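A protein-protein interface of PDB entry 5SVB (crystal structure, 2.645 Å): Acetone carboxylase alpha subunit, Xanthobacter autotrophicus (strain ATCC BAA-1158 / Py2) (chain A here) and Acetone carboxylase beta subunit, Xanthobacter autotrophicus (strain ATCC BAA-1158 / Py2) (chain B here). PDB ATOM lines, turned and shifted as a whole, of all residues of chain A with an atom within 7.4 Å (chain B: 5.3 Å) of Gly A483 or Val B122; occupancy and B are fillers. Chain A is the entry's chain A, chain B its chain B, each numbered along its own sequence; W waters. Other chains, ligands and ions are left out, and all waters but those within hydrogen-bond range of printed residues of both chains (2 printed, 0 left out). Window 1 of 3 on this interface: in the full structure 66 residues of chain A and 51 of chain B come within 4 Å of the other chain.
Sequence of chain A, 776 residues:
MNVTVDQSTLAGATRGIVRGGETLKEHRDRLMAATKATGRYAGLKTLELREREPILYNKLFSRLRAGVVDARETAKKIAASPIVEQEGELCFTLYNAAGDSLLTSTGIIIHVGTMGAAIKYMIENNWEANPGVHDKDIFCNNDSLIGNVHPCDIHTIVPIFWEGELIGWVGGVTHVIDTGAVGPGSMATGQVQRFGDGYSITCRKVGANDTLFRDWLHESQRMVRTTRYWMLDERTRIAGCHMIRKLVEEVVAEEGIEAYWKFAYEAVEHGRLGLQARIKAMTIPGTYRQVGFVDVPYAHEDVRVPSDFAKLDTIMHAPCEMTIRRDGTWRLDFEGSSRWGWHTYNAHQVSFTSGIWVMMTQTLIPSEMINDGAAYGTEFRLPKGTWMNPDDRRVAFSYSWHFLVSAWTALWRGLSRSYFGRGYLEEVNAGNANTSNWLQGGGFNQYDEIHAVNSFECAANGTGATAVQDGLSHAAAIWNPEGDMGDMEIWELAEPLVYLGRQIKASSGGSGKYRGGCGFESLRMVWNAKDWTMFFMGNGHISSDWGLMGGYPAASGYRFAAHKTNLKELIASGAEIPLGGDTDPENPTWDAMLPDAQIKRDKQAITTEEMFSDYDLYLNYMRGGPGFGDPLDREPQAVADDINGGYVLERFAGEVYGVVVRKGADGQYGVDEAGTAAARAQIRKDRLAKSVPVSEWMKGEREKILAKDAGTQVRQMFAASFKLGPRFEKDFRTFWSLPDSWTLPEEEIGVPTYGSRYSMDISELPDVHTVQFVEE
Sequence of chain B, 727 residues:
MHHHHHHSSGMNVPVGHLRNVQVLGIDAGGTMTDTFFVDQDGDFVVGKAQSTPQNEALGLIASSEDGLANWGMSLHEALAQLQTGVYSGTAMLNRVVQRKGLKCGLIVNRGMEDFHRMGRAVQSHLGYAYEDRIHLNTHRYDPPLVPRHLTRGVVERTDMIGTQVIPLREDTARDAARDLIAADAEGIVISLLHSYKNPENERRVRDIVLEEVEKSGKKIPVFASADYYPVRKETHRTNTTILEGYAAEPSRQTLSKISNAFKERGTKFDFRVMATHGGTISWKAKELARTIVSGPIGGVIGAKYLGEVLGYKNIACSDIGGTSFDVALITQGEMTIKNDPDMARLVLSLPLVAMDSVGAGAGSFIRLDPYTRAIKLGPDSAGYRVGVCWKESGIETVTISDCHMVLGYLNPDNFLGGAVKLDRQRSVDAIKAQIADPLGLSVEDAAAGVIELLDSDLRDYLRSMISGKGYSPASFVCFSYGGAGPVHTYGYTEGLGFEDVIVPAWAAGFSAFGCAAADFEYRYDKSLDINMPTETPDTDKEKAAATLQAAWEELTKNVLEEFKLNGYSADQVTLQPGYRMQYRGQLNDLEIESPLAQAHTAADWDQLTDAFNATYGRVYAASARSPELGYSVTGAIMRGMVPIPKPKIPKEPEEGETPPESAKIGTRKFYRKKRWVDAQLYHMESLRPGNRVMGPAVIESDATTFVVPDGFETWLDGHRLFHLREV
A ring nitrogen (NE2) of His B125 sits at hydrogen-bond distance from the backbone carbonyl oxygen (O) of Gly A483. The guanidinium group (NH2) of Arg B120 lies within salt-bridge range of the side-chain carboxylate (OD2) of Asp A484 (2.9 Å). The backbone carbonyl oxygen of Ala B121 sits close to the backbone carbonyl oxygen of Gly A483 (3.5 Å). A ring nitrogen (ND1) of His B139 sits close to the backbone carbonyl oxygen (O) of Pro A481 (3.5 Å). O of Gly A483 sits at hydrogen-bond distance from N of Val B122 (3.3 Å). The backbone NH (N) of Met A485 lies within hydrogen-bond range of the backbone carbonyl oxygen (O) of Arg B120, 2.9 Å away.
The side-chain carboxylate (OD1) of Asp A484 is in hydrogen-bond range of the backbone NH (N) of Gly A486 (2.9 Å). O of Ala B121 sits at hydrogen-bond distance from OG of Ser B124 (2.6 Å). The side-chain amide oxygen (OD1) of Asn A480 sits at hydrogen-bond distance from the backbone NH (N) of Glu A482.
Among the printed residues, merely in contact across the chains: Ala A460 with Ala B121 (3.7 Å), His A474 with Ala B121 (3.1 Å), Glu A482 with His B125 (3.4 Å), Asp A484 with Val B122 (3.96 Å) and Gly A486 with Arg B120 (3.5 Å).
Printed residues of chain A within 4 Å of Val B122: Gly A483 and Asp A484. Printed residues of chain B within 4 Å of Glu A482: His B125 (3.4 Å). Printed residues of chain B within 4 Å of Asp A484: Arg B120 (2.9 Å) and Val B122 (3.96 Å). Printed residues of chain A within 4 Å of His B139: Pro A481. Of the printed residues of chain A, Arg B120 touches Asp A484 (2.9 Å), Met A485 (2.9 Å) and Gly A486 (3.5 Å). Ala A459 touches none of the printed residues of chain B. Val B347 touches none of the printed residues of chain A. The nearest residue of chain A that does not touch Val B122 is Met A485 (5.1 Å). The nearest printed residue of chain B that does not touch Glu A482 is His B139 (4.3 Å).
Of the 10 printed residues of chain B, 5 touch a printed residue of chain A. Hydrophobic or aromatic side chains of chain B that line the printed part of chain A: Ala B121, Val B122, His B125 and His B139. Printed residues of chain A that touch a printed residue of chain B: Ala A460, His A474, Pro A481, Glu A482, Gly A483, Asp A484, Met A485 and Gly A486.
Water W2 lies within hydrogen-bond range of a ring nitrogen (ND1) of His B139 (2.5 Å), the side-chain hydroxyl (OG) of Ser B124 (2.7 Å) and the backbone carbonyl oxygen (O) of Ala A475 (2.9 Å). Water W1 lies within hydrogen-bond range of the backbone NH (N) of Arg B120 (3.0 Å) and the side-chain sulfur (SD) of Met A485 (3.8 Å).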
ATOM      1  N   ALA A 459      27.365   7.271  10.048  1.00  0.00           N
ATOM      2  CA  ALA A 459      27.408   7.094  11.490  1.00  0.00           C
ATOM      3  C   ALA A 459      27.965   5.736  11.890  1.00  0.00           C
ATOM      4  O   ALA A 459      28.113   5.476  13.088  1.00  0.00           O
ATOM      5  CB  ALA A 459      26.008   7.261  12.080  1.00  0.00           C
ATOM      6  N   ALA A 460      28.276   4.871  10.921  1.00  0.00           N
ATOM      7  CA  ALA A 460      28.725   3.509  11.184  1.00  0.00           C
ATOM      8  C   ALA A 460      29.938   3.219  10.297  1.00  0.00           C
ATOM      9  O   ALA A 460      29.854   2.487   9.309  1.00  0.00           O
ATOM     10  CB  ALA A 460      27.599   2.507  10.944  1.00  0.00           C
ATOM     11  N   ASN A 461      31.073   3.804  10.657  1.00  0.00           N
ATOM     12  CA  ASN A 461      32.334   3.557   9.979  1.00  0.00           C
ATOM     13  C   ASN A 461      33.117   2.473  10.707  1.00  0.00           C
ATOM     14  O   ASN A 461      32.740   2.010  11.784  1.00  0.00           O
ATOM     15  CB  ASN A 461      33.161   4.840   9.899  1.00  0.00           C
ATOM     16  CG  ASN A 461      32.438   5.956   9.186  1.00  0.00           C
ATOM     17  OD1 ASN A 461      32.367   5.979   7.960  1.00  0.00           O
ATOM     18  ND2 ASN A 461      31.903   6.898   9.951  1.00  0.00           N
ATOM     19  N   HIS A 474      31.956  -1.231  10.440  1.00  0.00           N
ATOM     20  CA  HIS A 474      30.684  -0.521  10.307  1.00  0.00           C
ATOM     21  C   HIS A 474      30.002  -0.354  11.662  1.00  0.00           C
ATOM     22  O   HIS A 474      28.868  -0.779  11.878  1.00  0.00           O
ATOM     23  CB  HIS A 474      29.766  -1.245   9.323  1.00  0.00           C
ATOM     24  CG  HIS A 474      29.625  -2.708   9.600  1.00  0.00           C
ATOM     25  ND1 HIS A 474      28.898  -3.196  10.664  1.00  0.00           N
ATOM     26  CD2 HIS A 474      30.142  -3.789   8.971  1.00  0.00           C
ATOM     27  CE1 HIS A 474      28.965  -4.515  10.672  1.00  0.00           C
ATOM     28  NE2 HIS A 474      29.714  -4.900   9.655  1.00  0.00           N
ATOM     29  N   ALA A 475      30.715   0.294  12.583  1.00  0.00           N
ATOM     30  CA  ALA A 475      30.314   0.264  13.983  1.00  0.00           C
ATOM     31  C   ALA A 475      30.188   1.637  14.627  1.00  0.00           C
ATOM     32  O   ALA A 475      29.424   1.796  15.584  1.00  0.00           O
ATOM     33  CB  ALA A 475      31.306  -0.573  14.782  1.00  0.00           C
ATOM     34  N   ALA A 476      30.923   2.633  14.148  1.00  0.00           N
ATOM     35  CA  ALA A 476      30.925   3.910  14.845  1.00  0.00           C
ATOM     36  C   ALA A 476      31.510   4.995  13.957  1.00  0.00           C
ATOM     37  O   ALA A 476      32.135   4.724  12.931  1.00  0.00           O
ATOM     38  CB  ALA A 476      31.712   3.818  16.156  1.00  0.00           C
ATOM     39  N   ALA A 477      31.281   6.235  14.373  1.00  0.00           N
ATOM     40  CA  ALA A 477      31.949   7.409  13.843  1.00  0.00           C
ATOM     41  C   ALA A 477      32.687   8.099  14.981  1.00  0.00           C
ATOM     42  O   ALA A 477      32.459   7.817  16.160  1.00  0.00           O
ATOM     43  CB  ALA A 477      30.949   8.369  13.187  1.00  0.00           C
ATOM     44  N   ASN A 480      30.405  10.085  17.200  1.00  0.00           N
ATOM     45  CA  ASN A 480      29.344   9.328  17.849  1.00  0.00           C
ATOM     46  C   ASN A 480      29.746   7.863  17.973  1.00  0.00           C
ATOM     47  O   ASN A 480      29.631   7.108  17.000  1.00  0.00           O
ATOM     48  CB  ASN A 480      28.034   9.442  17.071  1.00  0.00           C
ATOM     49  CG  ASN A 480      26.850   8.918  17.855  1.00  0.00           C
ATOM     50  OD1 ASN A 480      27.013   8.298  18.904  1.00  0.00           O
ATOM     51  ND2 ASN A 480      25.650   9.163  17.349  1.00  0.00           N
ATOM     52  N   PRO A 481      30.222   7.419  19.140  1.00  0.00           N
ATOM     53  CA  PRO A 481      30.572   5.998  19.288  1.00  0.00           C
ATOM     54  C   PRO A 481      29.373   5.069  19.272  1.00  0.00           C
ATOM     55  O   PRO A 481      29.534   3.889  18.945  1.00  0.00           O
ATOM     56  CB  PRO A 481      31.297   5.954  20.640  1.00  0.00           C
ATOM     57  CG  PRO A 481      30.780   7.127  21.377  1.00  0.00           C
ATOM     58  CD  PRO A 481      30.536   8.188  20.356  1.00  0.00           C
ATOM     59  N   GLU A 482      28.178   5.558  19.609  1.00  0.00           N
ATOM     60  CA  GLU A 482      26.965   4.740  19.579  1.00  0.00           C
ATOM     61  C   GLU A 482      26.450   4.665  18.140  1.00  0.00           C
ATOM     62  O   GLU A 482      25.410   5.217  17.775  1.00  0.00           O
ATOM     63  CB  GLU A 482      25.915   5.313  20.520  1.00  0.00           C
ATOM     64  CG  GLU A 482      26.303   5.247  21.985  1.00  0.00           C
ATOM     65  CD  GLU A 482      25.340   6.001  22.880  1.00  0.00           C
ATOM     66  OE1 GLU A 482      24.192   5.540  23.039  1.00  0.00           O
ATOM     67  OE2 GLU A 482      25.729   7.060  23.416  1.00  0.00           O
ATOM     68  N   GLY A 483      27.208   3.947  17.315  1.00  0.00           N
ATOM     69  CA  GLY A 483      26.927   3.919  15.889  1.00  0.00           C
ATOM     70  C   GLY A 483      25.653   3.153  15.585  1.00  0.00           C
ATOM     71  O   GLY A 483      25.462   2.022  16.047  1.00  0.00           O
ATOM     72  N   ASP A 484      24.772   3.770  14.804  1.00  0.00           N
ATOM     73  CA  ASP A 484      23.574   3.118  14.303  1.00  0.00           C
ATOM     74  C   ASP A 484      23.482   3.350  12.803  1.00  0.00           C
ATOM     75  O   ASP A 484      23.691   4.464  12.315  1.00  0.00           O
ATOM     76  CB  ASP A 484      22.310   3.634  14.990  1.00  0.00           C
ATOM     77  CG  ASP A 484      21.118   2.718  14.780  1.00  0.00           C
ATOM     78  OD1 ASP A 484      21.066   2.028  13.741  1.00  0.00           O
ATOM     79  OD2 ASP A 484      20.233   2.686  15.658  1.00  0.00           O
ATOM     80  N   MET A 485      23.155   2.290  12.085  1.00  0.00           N
ATOM     81  CA  MET A 485      23.185   2.281  10.635  1.00  0.00           C
ATOM     82  C   MET A 485      21.831   2.660  10.050  1.00  0.00           C
ATOM     83  O   MET A 485      21.740   3.127   8.915  1.00  0.00           O
ATOM     84  CB  MET A 485      23.599   0.892  10.167  1.00  0.00           C
ATOM     85  CG  MET A 485      23.913   0.757   8.711  1.00  0.00           C
ATOM     86  SD  MET A 485      24.258  -1.113   8.353  1.00  0.00           S
ATOM     87  CE  MET A 485      25.949  -1.301   9.293  1.00  0.00           C
ATOM     88  N   GLY A 486      20.784   2.453  10.836  1.00  0.00           N
ATOM     89  CA  GLY A 486      19.429   2.658  10.378  1.00  0.00           C
ATOM     90  C   GLY A 486      18.917   1.489   9.554  1.00  0.00           C
ATOM     91  O   GLY A 486      19.673   0.705   8.986  1.00  0.00           O
ATOM     92  N   GLY B 119      24.408  -6.435  12.029  1.00  0.00           N
ATOM     93  CA  GLY B 119      23.764  -6.014  13.256  1.00  0.00           C
ATOM     94  C   GLY B 119      23.369  -4.560  13.282  1.00  0.00           C
ATOM     95  O   GLY B 119      23.195  -3.993  14.362  1.00  0.00           O
ATOM     96  N   ARG B 120      23.233  -3.930  12.115  1.00  0.00           N
ATOM     97  CA  ARG B 120      22.850  -2.525  12.009  1.00  0.00           C
ATOM     98  C   ARG B 120      23.786  -1.615  12.800  1.00  0.00           C
ATOM     99  O   ARG B 120      23.438  -0.467  13.089  1.00  0.00           O
ATOM    100  CB  ARG B 120      21.404  -2.317  12.466  1.00  0.00           C
ATOM    101  CG  ARG B 120      20.653  -1.278  11.662  1.00  0.00           C
ATOM    102  CD  ARG B 120      19.270  -1.062  12.226  1.00  0.00           C
ATOM    103  NE  ARG B 120      19.308  -0.293  13.464  1.00  0.00           N
ATOM    104  CZ  ARG B 120      18.366  -0.331  14.398  1.00  0.00           C
ATOM    105  NH1 ARG B 120      17.309  -1.114  14.253  1.00  0.00           N
ATOM    106  NH2 ARG B 120      18.484   0.409  15.490  1.00  0.00           N
ATOM    107  N   ALA B 121      24.965  -2.120  13.163  1.00  0.00           N
ATOM    108  CA  ALA B 121      25.960  -1.386  13.939  1.00  0.00           C
ATOM    109  C   ALA B 121      25.569  -1.256  15.408  1.00  0.00           C
ATOM    110  O   ALA B 121      26.434  -1.314  16.288  1.00  0.00           O
ATOM    111  CB  ALA B 121      26.207   0.003  13.344  1.00  0.00           C
ATOM    112  N   VAL B 122      24.278  -1.088  15.694  1.00  0.00           N
ATOM    113  CA  VAL B 122      23.862  -0.777  17.056  1.00  0.00           C
ATOM    114  C   VAL B 122      24.069  -1.967  17.983  1.00  0.00           C
ATOM    115  O   VAL B 122      24.262  -1.791  19.191  1.00  0.00           O
ATOM    116  CB  VAL B 122      22.396  -0.312  17.068  1.00  0.00           C
ATOM    117  CG1 VAL B 122      21.458  -1.466  16.731  1.00  0.00           C
ATOM    118  CG2 VAL B 122      22.054   0.297  18.415  1.00  0.00           C
ATOM    119  N   GLN B 123      24.028  -3.185  17.456  1.00  0.00           N
ATOM    120  CA  GLN B 123      24.152  -4.361  18.306  1.00  0.00           C
ATOM    121  C   GLN B 123      25.553  -4.538  18.869  1.00  0.00           C
ATOM    122  O   GLN B 123      25.783  -5.503  19.608  1.00  0.00           O
ATOM    123  CB  GLN B 123      23.736  -5.608  17.526  1.00  0.00           C
ATOM    124  CG  GLN B 123      22.249  -5.635  17.203  1.00  0.00           C
ATOM    125  CD  GLN B 123      21.794  -6.884  16.472  1.00  0.00           C
ATOM    126  OE1 GLN B 123      20.595  -7.109  16.323  1.00  0.00           O
ATOM    127  NE2 GLN B 123      22.738  -7.699  16.010  1.00  0.00           N
ATOM    128  N   SER B 124      26.485  -3.643  18.552  1.00  0.00           N
ATOM    129  CA  SER B 124      27.814  -3.677  19.143  1.00  0.00           C
ATOM    130  C   SER B 124      27.877  -2.964  20.487  1.00  0.00           C
ATOM    131  O   SER B 124      28.928  -2.994  21.136  1.00  0.00           O
ATOM    132  CB  SER B 124      28.832  -3.057  18.182  1.00  0.00           C
ATOM    133  OG  SER B 124      28.464  -1.739  17.825  1.00  0.00           O
ATOM    134  N   HIS B 125      26.778  -2.331  20.923  1.00  0.00           N
ATOM    135  CA  HIS B 125      26.774  -1.603  22.188  1.00  0.00           C
ATOM    136  C   HIS B 125      25.395  -1.596  22.842  1.00  0.00           C
ATOM    137  O   HIS B 125      25.075  -0.670  23.595  1.00  0.00           O
ATOM    138  CB  HIS B 125      27.257  -0.165  21.982  1.00  0.00           C
ATOM    139  CG  HIS B 125      26.501   0.581  20.928  1.00  0.00           C
ATOM    140  ND1 HIS B 125      25.341   1.276  21.194  1.00  0.00           N
ATOM    141  CD2 HIS B 125      26.737   0.737  19.605  1.00  0.00           C
ATOM    142  CE1 HIS B 125      24.897   1.829  20.080  1.00  0.00           C
ATOM    143  NE2 HIS B 125      25.726   1.517  19.101  1.00  0.00           N
ATOM    144  N   LEU B 126      24.572  -2.605  22.572  1.00  0.00           N
ATOM    145  CA  LEU B 126      23.279  -2.714  23.230  1.00  0.00           C
ATOM    146  C   LEU B 126      23.447  -3.263  24.639  1.00  0.00           C
ATOM    147  O   LEU B 126      24.263  -4.156  24.883  1.00  0.00           O
ATOM    148  CB  LEU B 126      22.341  -3.617  22.429  1.00  0.00           C
ATOM    149  CG  LEU B 126      21.768  -3.038  21.136  1.00  0.00           C
ATOM    150  CD1 LEU B 126      21.028  -4.114  20.367  1.00  0.00           C
ATOM    151  CD2 LEU B 126      20.846  -1.869  21.426  1.00  0.00           C
ATOM    152  N   HIS B 139      33.043  -1.761  22.914  1.00  0.00           N
ATOM    153  CA  HIS B 139      32.076  -2.220  21.931  1.00  0.00           C
ATOM    154  C   HIS B 139      32.500  -3.565  21.364  1.00  0.00           C
ATOM    155  O   HIS B 139      33.688  -3.876  21.261  1.00  0.00           O
ATOM    156  CB  HIS B 139      31.929  -1.189  20.814  1.00  0.00           C
ATOM    157  CG  HIS B 139      31.249   0.071  21.250  1.00  0.00           C
ATOM    158  ND1 HIS B 139      30.545   0.877  20.383  1.00  0.00           N
ATOM    159  CD2 HIS B 139      31.162   0.661  22.465  1.00  0.00           C
ATOM    160  CE1 HIS B 139      30.054   1.909  21.045  1.00  0.00           C
ATOM    161  NE2 HIS B 139      30.415   1.802  22.310  1.00  0.00           N
ATOM    162  N   VAL B 347      18.086  -6.498  18.087  1.00  0.00           N
ATOM    163  CA  VAL B 347      16.896  -5.716  17.787  1.00  0.00           C
ATOM    164  C   VAL B 347      15.789  -6.670  17.364  1.00  0.00           C
ATOM    165  O   VAL B 347      16.000  -7.556  16.527  1.00  0.00           O
ATOM    166  CB  VAL B 347      17.193  -4.670  16.701  1.00  0.00           C
ATOM    167  CG1 VAL B 347      18.242  -3.689  17.189  1.00  0.00           C
ATOM    168  CG2 VAL B 347      17.648  -5.330  15.414  1.00  0.00           C
HETATM  169  O   HOH W   1      21.971  -3.935   9.368  1.00  0.00           O
HETATM  170  O   HOH W   2      30.089   0.394  17.996  1.00  0.00           O
